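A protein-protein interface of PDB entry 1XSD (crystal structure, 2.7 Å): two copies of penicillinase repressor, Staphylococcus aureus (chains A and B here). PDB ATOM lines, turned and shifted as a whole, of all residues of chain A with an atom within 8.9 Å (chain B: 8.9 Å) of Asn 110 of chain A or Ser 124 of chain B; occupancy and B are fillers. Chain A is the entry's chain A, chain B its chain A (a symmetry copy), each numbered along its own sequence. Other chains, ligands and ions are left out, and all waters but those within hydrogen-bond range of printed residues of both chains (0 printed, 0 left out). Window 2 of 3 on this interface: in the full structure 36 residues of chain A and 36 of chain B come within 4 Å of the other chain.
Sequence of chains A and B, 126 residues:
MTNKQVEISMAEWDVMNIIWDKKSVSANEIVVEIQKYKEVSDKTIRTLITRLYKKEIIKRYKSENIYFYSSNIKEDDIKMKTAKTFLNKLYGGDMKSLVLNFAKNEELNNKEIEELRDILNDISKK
OG of Ser 124 of chain B sits at hydrogen-bond distance from OE1 of Glu 114 of chain A, 2.6 Å away.
No residue of chain B comes within 4 Å of Asn 109 of chain A. Asn 110 of chain A touches just one residue of chain B: Ser 124 (3.6 Å). Of chain B, only Ser 124 comes within 4 Å of Ile 113 of chain A. Printed residues of chain B within 4 Å of Arg 117 of chain A: Leu 120 (3.7 Å) and Asn 121 (3.4 Å). Arg 117 of chain B touches none of the printed residues of chain A. Of the printed residues of chain A, Leu 120 of chain B touches Leu 116 and Arg 117. Printed residues of chain A within 4 Å of Asn 121 of chain B: Arg 117 (3.4 Å). Asp 122 of chain B touches none of the printed residues of chain A. Of chain A, only Asn 110 (3.6 Å), Ile 113 (3.9 Å) and Glu 114 (2.6 Å) come within 4 Å of Ser 124 of chain B. The nearest residue of chain B that does not touch Asn 110 of chain A is Ile 123 of chain B (5.0 Å). The nearest residue of chain A that does not touch Ser 124 of chain B is Arg 117 of chain A (4.2 Å). The nearest printed residue of chain B that does not touch Arg 117 of chain A is Ser 124 of chain B (4.2 Å).
Positions printed for both chains: 117 and 118.
Among the printed residues, pairs that only touch across the chains: Ala 103 of chain A with Ile 123 of chain B, Asn 110 of chain A with Ser 124 of chain B, Ile 113 of chain A with Ser 124 of chain B, Leu 116 of chain A with Leu 120 of chain B, Arg 117 of chain A with Leu 120 of chain B and Arg 117 of chain A with Asn 121 of chain B.
Of the 15 printed residues of chain A, 6 touch a printed residue of chain B. Printed residues of chain A that touch a printed residue of chain B: Ala 103, Asn 110, Ile 113, Glu 114, Leu 116 and Arg 117. Hydrophobic or aromatic side chains of chain A that line the printed part of chain B: Ala 103, Ile 113 and Leu 116. Of the 10 printed residues of chain B, 4 touch a printed residue of chain A. Along chain B the printed residues that touch a printed residue of chain A span positions 120 to 124.
The guanidinium group (NH1) of Arg 117 of chain A lies within salt-bridge range of the side-chain carboxylate (OE2) of Glu 114 of chain A (2.9 Å).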
ATOM      1  N   LEU A 100      13.109 -31.540 -11.994  1.00  0.00           N
ATOM      2  CA  LEU A 100      11.789 -30.972 -11.868  1.00  0.00           C
ATOM      3  C   LEU A 100      11.131 -31.362 -10.522  1.00  0.00           C
ATOM      4  O   LEU A 100      10.398 -30.566  -9.943  1.00  0.00           O
ATOM      5  CB  LEU A 100      10.939 -31.412 -13.057  1.00  0.00           C
ATOM      6  CG  LEU A 100       9.727 -30.509 -13.226  1.00  0.00           C
ATOM      7  CD1 LEU A 100      10.170 -29.052 -12.950  1.00  0.00           C
ATOM      8  CD2 LEU A 100       9.086 -30.712 -14.625  1.00  0.00           C
ATOM      9  N   ALA A 103      12.639 -28.761  -7.963  1.00  0.00           N
ATOM     10  CA  ALA A 103      12.005 -27.460  -7.916  1.00  0.00           C
ATOM     11  C   ALA A 103      10.618 -27.635  -7.243  1.00  0.00           C
ATOM     12  O   ALA A 103      10.342 -27.031  -6.200  1.00  0.00           O
ATOM     13  CB  ALA A 103      11.878 -26.896  -9.323  1.00  0.00           C
ATOM     14  N   GLU A 106      10.080 -27.855  -3.798  1.00  0.00           N
ATOM     15  CA  GLU A 106      10.697 -26.649  -3.246  1.00  0.00           C
ATOM     16  C   GLU A 106      11.910 -26.944  -2.404  1.00  0.00           C
ATOM     17  O   GLU A 106      12.014 -26.515  -1.260  1.00  0.00           O
ATOM     18  CB  GLU A 106       9.683 -25.881  -2.401  1.00  0.00           C
ATOM     19  CG  GLU A 106       8.375 -25.623  -3.124  1.00  0.00           C
ATOM     20  CD  GLU A 106       7.292 -25.068  -2.210  1.00  0.00           C
ATOM     21  OE1 GLU A 106       7.566 -24.034  -1.554  1.00  0.00           O
ATOM     22  OE2 GLU A 106       6.180 -25.661  -2.158  1.00  0.00           O
ATOM     23  N   GLU A 107      12.823 -27.691  -2.997  1.00  0.00           N
ATOM     24  CA  GLU A 107      14.067 -28.054  -2.361  1.00  0.00           C
ATOM     25  C   GLU A 107      15.151 -27.167  -2.959  1.00  0.00           C
ATOM     26  O   GLU A 107      16.344 -27.400  -2.754  1.00  0.00           O
ATOM     27  CB  GLU A 107      14.390 -29.519  -2.646  1.00  0.00           C
ATOM     28  CG  GLU A 107      13.523 -30.514  -1.912  1.00  0.00           C
ATOM     29  CD  GLU A 107      13.677 -30.406  -0.410  1.00  0.00           C
ATOM     30  OE1 GLU A 107      14.817 -30.164   0.051  1.00  0.00           O
ATOM     31  OE2 GLU A 107      12.659 -30.575   0.297  1.00  0.00           O
ATOM     32  N   LEU A 108      14.734 -26.158  -3.716  1.00  0.00           N
ATOM     33  CA  LEU A 108      15.682 -25.237  -4.338  1.00  0.00           C
ATOM     34  C   LEU A 108      15.176 -23.794  -4.380  1.00  0.00           C
ATOM     35  O   LEU A 108      14.086 -23.520  -4.908  1.00  0.00           O
ATOM     36  CB  LEU A 108      16.018 -25.678  -5.770  1.00  0.00           C
ATOM     37  CG  LEU A 108      16.552 -27.088  -6.040  1.00  0.00           C
ATOM     38  CD1 LEU A 108      16.982 -27.182  -7.499  1.00  0.00           C
ATOM     39  CD2 LEU A 108      17.736 -27.402  -5.138  1.00  0.00           C
ATOM     40  N   ASN A 109      15.965 -22.882  -3.807  1.00  0.00           N
ATOM     41  CA  ASN A 109      15.631 -21.467  -3.826  1.00  0.00           C
ATOM     42  C   ASN A 109      16.180 -20.892  -5.122  1.00  0.00           C
ATOM     43  O   ASN A 109      17.236 -21.321  -5.598  1.00  0.00           O
ATOM     44  CB  ASN A 109      16.257 -20.718  -2.656  1.00  0.00           C
ATOM     45  CG  ASN A 109      16.154 -19.201  -2.832  1.00  0.00           C
ATOM     46  OD1 ASN A 109      16.953 -18.595  -3.573  1.00  0.00           O
ATOM     47  ND2 ASN A 109      15.150 -18.578  -2.177  1.00  0.00           N
ATOM     48  N   ASN A 110      15.466 -19.914  -5.679  1.00  0.00           N
ATOM     49  CA  ASN A 110      15.864 -19.278  -6.941  1.00  0.00           C
ATOM     50  C   ASN A 110      17.362 -18.927  -6.999  1.00  0.00           C
ATOM     51  O   ASN A 110      17.943 -18.818  -8.093  1.00  0.00           O
ATOM     52  CB  ASN A 110      15.021 -18.015  -7.204  1.00  0.00           C
ATOM     53  CG  ASN A 110      15.235 -17.445  -8.615  1.00  0.00           C
ATOM     54  OD1 ASN A 110      14.649 -17.928  -9.598  1.00  0.00           O
ATOM     55  ND2 ASN A 110      16.088 -16.420  -8.716  1.00  0.00           N
ATOM     56  N   LYS A 111      17.989 -18.739  -5.841  1.00  0.00           N
ATOM     57  CA  LYS A 111      19.403 -18.441  -5.860  1.00  0.00           C
ATOM     58  C   LYS A 111      20.095 -19.691  -6.403  1.00  0.00           C
ATOM     59  O   LYS A 111      20.856 -19.620  -7.375  1.00  0.00           O
ATOM     60  CB  LYS A 111      19.923 -18.101  -4.465  1.00  0.00           C
ATOM     61  CG  LYS A 111      21.439 -17.863  -4.423  1.00  0.00           C
ATOM     62  CD  LYS A 111      21.927 -17.533  -3.020  1.00  0.00           C
ATOM     63  CE  LYS A 111      21.350 -16.188  -2.519  1.00  0.00           C
ATOM     64  NZ  LYS A 111      21.525 -15.945  -1.033  1.00  0.00           N
ATOM     65  N   GLU A 112      19.811 -20.840  -5.799  1.00  0.00           N
ATOM     66  CA  GLU A 112      20.413 -22.081  -6.256  1.00  0.00           C
ATOM     67  C   GLU A 112      19.856 -22.438  -7.632  1.00  0.00           C
ATOM     68  O   GLU A 112      20.563 -23.025  -8.469  1.00  0.00           O
ATOM     69  CB  GLU A 112      20.124 -23.190  -5.263  1.00  0.00           C
ATOM     70  CG  GLU A 112      20.541 -22.810  -3.883  1.00  0.00           C
ATOM     71  CD  GLU A 112      20.091 -23.805  -2.846  1.00  0.00           C
ATOM     72  OE1 GLU A 112      18.873 -24.111  -2.786  1.00  0.00           O
ATOM     73  OE2 GLU A 112      20.963 -24.276  -2.083  1.00  0.00           O
ATOM     74  N   ILE A 113      18.596 -22.073  -7.874  1.00  0.00           N
ATOM     75  CA  ILE A 113      17.972 -22.364  -9.161  1.00  0.00           C
ATOM     76  C   ILE A 113      18.713 -21.648 -10.259  1.00  0.00           C
ATOM     77  O   ILE A 113      18.878 -22.184 -11.352  1.00  0.00           O
ATOM     78  CB  ILE A 113      16.524 -21.882  -9.254  1.00  0.00           C
ATOM     79  CG1 ILE A 113      15.673 -22.491  -8.121  1.00  0.00           C
ATOM     80  CG2 ILE A 113      15.990 -22.233 -10.645  1.00  0.00           C
ATOM     81  CD1 ILE A 113      14.227 -21.949  -8.026  1.00  0.00           C
ATOM     82  N   GLU A 114      19.142 -20.424  -9.963  1.00  0.00           N
ATOM     83  CA  GLU A 114      19.868 -19.632 -10.941  1.00  0.00           C
ATOM     84  C   GLU A 114      21.316 -20.116 -11.061  1.00  0.00           C
ATOM     85  O   GLU A 114      21.813 -20.248 -12.186  1.00  0.00           O
ATOM     86  CB  GLU A 114      19.795 -18.130 -10.596  1.00  0.00           C
ATOM     87  CG  GLU A 114      20.140 -17.167 -11.779  1.00  0.00           C
ATOM     88  CD  GLU A 114      19.079 -17.107 -12.915  1.00  0.00           C
ATOM     89  OE1 GLU A 114      18.680 -18.177 -13.420  1.00  0.00           O
ATOM     90  OE2 GLU A 114      18.651 -15.991 -13.326  1.00  0.00           O
ATOM     91  N   GLU A 115      21.990 -20.394  -9.933  1.00  0.00           N
ATOM     92  CA  GLU A 115      23.383 -20.895  -9.980  1.00  0.00           C
ATOM     93  C   GLU A 115      23.379 -22.117 -10.858  1.00  0.00           C
ATOM     94  O   GLU A 115      24.259 -22.304 -11.692  1.00  0.00           O
ATOM     95  CB  GLU A 115      23.910 -21.354  -8.625  1.00  0.00           C
ATOM     96  CG  GLU A 115      23.954 -20.304  -7.583  1.00  0.00           C
ATOM     97  CD  GLU A 115      24.460 -20.857  -6.284  1.00  0.00           C
ATOM     98  OE1 GLU A 115      23.991 -21.953  -5.911  1.00  0.00           O
ATOM     99  OE2 GLU A 115      25.313 -20.204  -5.639  1.00  0.00           O
ATOM    100  N   LEU A 116      22.389 -22.973 -10.655  1.00  0.00           N
ATOM    101  CA  LEU A 116      22.311 -24.167 -11.470  1.00  0.00           C
ATOM    102  C   LEU A 116      22.175 -23.733 -12.921  1.00  0.00           C
ATOM    103  O   LEU A 116      23.111 -23.897 -13.706  1.00  0.00           O
ATOM    104  CB  LEU A 116      21.123 -25.025 -11.056  1.00  0.00           C
ATOM    105  CG  LEU A 116      21.369 -26.496 -11.370  1.00  0.00           C
ATOM    106  CD1 LEU A 116      22.584 -27.015 -10.602  1.00  0.00           C
ATOM    107  CD2 LEU A 116      20.145 -27.272 -11.006  1.00  0.00           C
ATOM    108  N   ARG A 117      21.017 -23.150 -13.253  1.00  0.00           N
ATOM    109  CA  ARG A 117      20.731 -22.664 -14.610  1.00  0.00           C
ATOM    110  C   ARG A 117      22.005 -22.059 -15.188  1.00  0.00           C
ATOM    111  O   ARG A 117      22.274 -22.166 -16.381  1.00  0.00           O
ATOM    112  CB  ARG A 117      19.611 -21.597 -14.601  1.00  0.00           C
ATOM    113  CG  ARG A 117      19.087 -21.202 -16.006  1.00  0.00           C
ATOM    114  CD  ARG A 117      18.990 -19.693 -16.198  1.00  0.00           C
ATOM    115  NE  ARG A 117      20.319 -19.099 -16.070  1.00  0.00           N
ATOM    116  CZ  ARG A 117      20.589 -17.795 -15.960  1.00  0.00           C
ATOM    117  NH1 ARG A 117      19.603 -16.898 -15.966  1.00  0.00           N
ATOM    118  NH2 ARG A 117      21.861 -17.397 -15.820  1.00  0.00           N
ATOM    119  N   ASP A 118      22.787 -21.428 -14.325  1.00  0.00           N
ATOM    120  CA  ASP A 118      24.033 -20.831 -14.754  1.00  0.00           C
ATOM    121  C   ASP A 118      24.905 -21.997 -15.217  1.00  0.00           C
ATOM    122  O   ASP A 118      24.782 -22.437 -16.355  1.00  0.00           O
ATOM    123  CB  ASP A 118      24.676 -20.091 -13.591  1.00  0.00           C
ATOM    124  CG  ASP A 118      25.720 -19.123 -14.036  1.00  0.00           C
ATOM    125  OD1 ASP A 118      26.429 -19.440 -15.018  1.00  0.00           O
ATOM    126  OD2 ASP A 118      25.841 -18.060 -13.391  1.00  0.00           O
ATOM    127  N   ARG B 117      19.060 -27.524 -19.813  1.00  0.00           N
ATOM    128  CA  ARG B 117      19.295 -26.075 -19.731  1.00  0.00           C
ATOM    129  C   ARG B 117      17.986 -25.353 -20.028  1.00  0.00           C
ATOM    130  O   ARG B 117      17.693 -24.309 -19.452  1.00  0.00           O
ATOM    131  CB  ARG B 117      20.376 -25.623 -20.741  1.00  0.00           C
ATOM    132  CG  ARG B 117      20.851 -24.157 -20.562  1.00  0.00           C
ATOM    133  CD  ARG B 117      20.887 -23.383 -21.875  1.00  0.00           C
ATOM    134  NE  ARG B 117      19.541 -23.316 -22.439  1.00  0.00           N
ATOM    135  CZ  ARG B 117      19.227 -22.913 -23.673  1.00  0.00           C
ATOM    136  NH1 ARG B 117      20.179 -22.518 -24.518  1.00  0.00           N
ATOM    137  NH2 ARG B 117      17.945 -22.931 -24.064  1.00  0.00           N
ATOM    138  N   ASP B 118      17.203 -25.925 -20.929  1.00  0.00           N
ATOM    139  CA  ASP B 118      15.926 -25.342 -21.278  1.00  0.00           C
ATOM    140  C   ASP B 118      15.086 -25.408 -20.003  1.00  0.00           C
ATOM    141  O   ASP B 118      15.198 -24.531 -19.153  1.00  0.00           O
ATOM    142  CB  ASP B 118      15.284 -26.142 -22.402  1.00  0.00           C
ATOM    143  CG  ASP B 118      14.195 -25.390 -23.089  1.00  0.00           C
ATOM    144  OD1 ASP B 118      13.475 -24.639 -22.393  1.00  0.00           O
ATOM    145  OD2 ASP B 118      14.052 -25.568 -24.318  1.00  0.00           O
ATOM    146  N   ILE B 119      14.257 -26.443 -19.874  1.00  0.00           N
ATOM    147  CA  ILE B 119      13.410 -26.673 -18.688  1.00  0.00           C
ATOM    148  C   ILE B 119      13.904 -25.947 -17.409  1.00  0.00           C
ATOM    149  O   ILE B 119      13.122 -25.337 -16.669  1.00  0.00           O
ATOM    150  CB  ILE B 119      13.329 -28.206 -18.397  1.00  0.00           C
ATOM    151  CG1 ILE B 119      12.552 -28.475 -17.121  1.00  0.00           C
ATOM    152  CG2 ILE B 119      14.728 -28.794 -18.217  1.00  0.00           C
ATOM    153  CD1 ILE B 119      12.782 -29.870 -16.598  1.00  0.00           C
ATOM    154  N   LEU B 120      15.212 -26.036 -17.173  1.00  0.00           N
ATOM    155  CA  LEU B 120      15.879 -25.434 -16.023  1.00  0.00           C
ATOM    156  C   LEU B 120      15.882 -23.918 -16.108  1.00  0.00           C
ATOM    157  O   LEU B 120      15.733 -23.233 -15.098  1.00  0.00           O
ATOM    158  CB  LEU B 120      17.320 -25.936 -15.954  1.00  0.00           C
ATOM    159  CG  LEU B 120      18.226 -25.416 -14.837  1.00  0.00           C
ATOM    160  CD1 LEU B 120      17.504 -25.569 -13.488  1.00  0.00           C
ATOM    161  CD2 LEU B 120      19.561 -26.191 -14.859  1.00  0.00           C
ATOM    162  N   ASN B 121      16.098 -23.392 -17.311  1.00  0.00           N
ATOM    163  CA  ASN B 121      16.080 -21.948 -17.520  1.00  0.00           C
ATOM    164  C   ASN B 121      14.612 -21.543 -17.345  1.00  0.00           C
ATOM    165  O   ASN B 121      14.295 -20.467 -16.830  1.00  0.00           O
ATOM    166  CB  ASN B 121      16.597 -21.619 -18.930  1.00  0.00           C
ATOM    167  CG  ASN B 121      16.101 -20.272 -19.443  1.00  0.00           C
ATOM    168  OD1 ASN B 121      15.071 -20.190 -20.129  1.00  0.00           O
ATOM    169  ND2 ASN B 121      16.822 -19.206 -19.098  1.00  0.00           N
ATOM    170  N   ASP B 122      13.739 -22.458 -17.755  1.00  0.00           N
ATOM    171  CA  ASP B 122      12.309 -22.302 -17.680  1.00  0.00           C
ATOM    172  C   ASP B 122      11.835 -22.228 -16.214  1.00  0.00           C
ATOM    173  O   ASP B 122      10.821 -21.598 -15.912  1.00  0.00           O
ATOM    174  CB  ASP B 122      11.670 -23.480 -18.441  1.00  0.00           C
ATOM    175  CG  ASP B 122      10.136 -23.436 -18.471  1.00  0.00           C
ATOM    176  OD1 ASP B 122       9.562 -22.320 -18.464  1.00  0.00           O
ATOM    177  OD2 ASP B 122       9.508 -24.525 -18.532  1.00  0.00           O
ATOM    178  N   ILE B 123      12.575 -22.845 -15.299  1.00  0.00           N
ATOM    179  CA  ILE B 123      12.184 -22.831 -13.886  1.00  0.00           C
ATOM    180  C   ILE B 123      12.550 -21.524 -13.211  1.00  0.00           C
ATOM    181  O   ILE B 123      11.818 -21.023 -12.345  1.00  0.00           O
ATOM    182  CB  ILE B 123      12.863 -23.960 -13.087  1.00  0.00           C
ATOM    183  CG1 ILE B 123      12.589 -25.317 -13.751  1.00  0.00           C
ATOM    184  CG2 ILE B 123      12.373 -23.926 -11.635  1.00  0.00           C
ATOM    185  CD1 ILE B 123      13.670 -26.360 -13.472  1.00  0.00           C
ATOM    186  N   SER B 124      13.705 -20.996 -13.606  1.00  0.00           N
ATOM    187  CA  SER B 124      14.216 -19.739 -13.082  1.00  0.00           C
ATOM    188  C   SER B 124      13.291 -18.604 -13.508  1.00  0.00           C
ATOM    189  O   SER B 124      13.239 -17.563 -12.853  1.00  0.00           O
ATOM    190  CB  SER B 124      15.621 -19.479 -13.621  1.00  0.00           C
ATOM    191  OG  SER B 124      16.150 -18.283 -13.068  1.00  0.00           O
ATOM    192  N   LYS B 125      12.574 -18.828 -14.613  1.00  0.00           N
ATOM    193  CA  LYS B 125      11.631 -17.862 -15.188  1.00  0.00           C
ATOM    194  C   LYS B 125      10.391 -17.752 -14.319  1.00  0.00           C
ATOM    195  O   LYS B 125       9.652 -18.728 -14.144  1.00  0.00           O
ATOM    196  CB  LYS B 125      11.223 -18.280 -16.612  1.00  0.00           C
ATOM    197  CG  LYS B 125      12.395 -18.328 -17.592  1.00  0.00           C
ATOM    198  CD  LYS B 125      11.969 -18.559 -19.044  1.00  0.00           C
ATOM    199  CE  LYS B 125      11.279 -19.904 -19.258  1.00  0.00           C
ATOM    200  NZ  LYS B 125      11.088 -20.234 -20.699  1.00  0.00           N
ATOM    201  N   LYS B 126      10.183 -16.558 -13.768  1.00  0.00           N
ATOM    202  CA  LYS B 126       9.037 -16.297 -12.908  1.00  0.00           C
ATOM    203  C   LYS B 126       7.942 -15.569 -13.681  1.00  0.00           C
ATOM    204  O   LYS B 126       8.101 -15.470 -14.919  1.00  0.00           O
ATOM    205  CB  LYS B 126       9.466 -15.488 -11.673  1.00  0.00           C
ATOM    206  CG  LYS B 126      10.344 -14.286 -11.949  1.00  0.00           C
ATOM    207  CD  LYS B 126      10.822 -13.680 -10.637  1.00  0.00           C
ATOM    208  CE  LYS B 126      11.995 -12.728 -10.854  1.00  0.00           C
ATOM    209  NZ  LYS B 126      11.710 -11.631 -11.839  1.00  0.00           N
ATOM    210  OXT LYS B 126       6.944 -15.135 -13.055  1.00  0.00           O
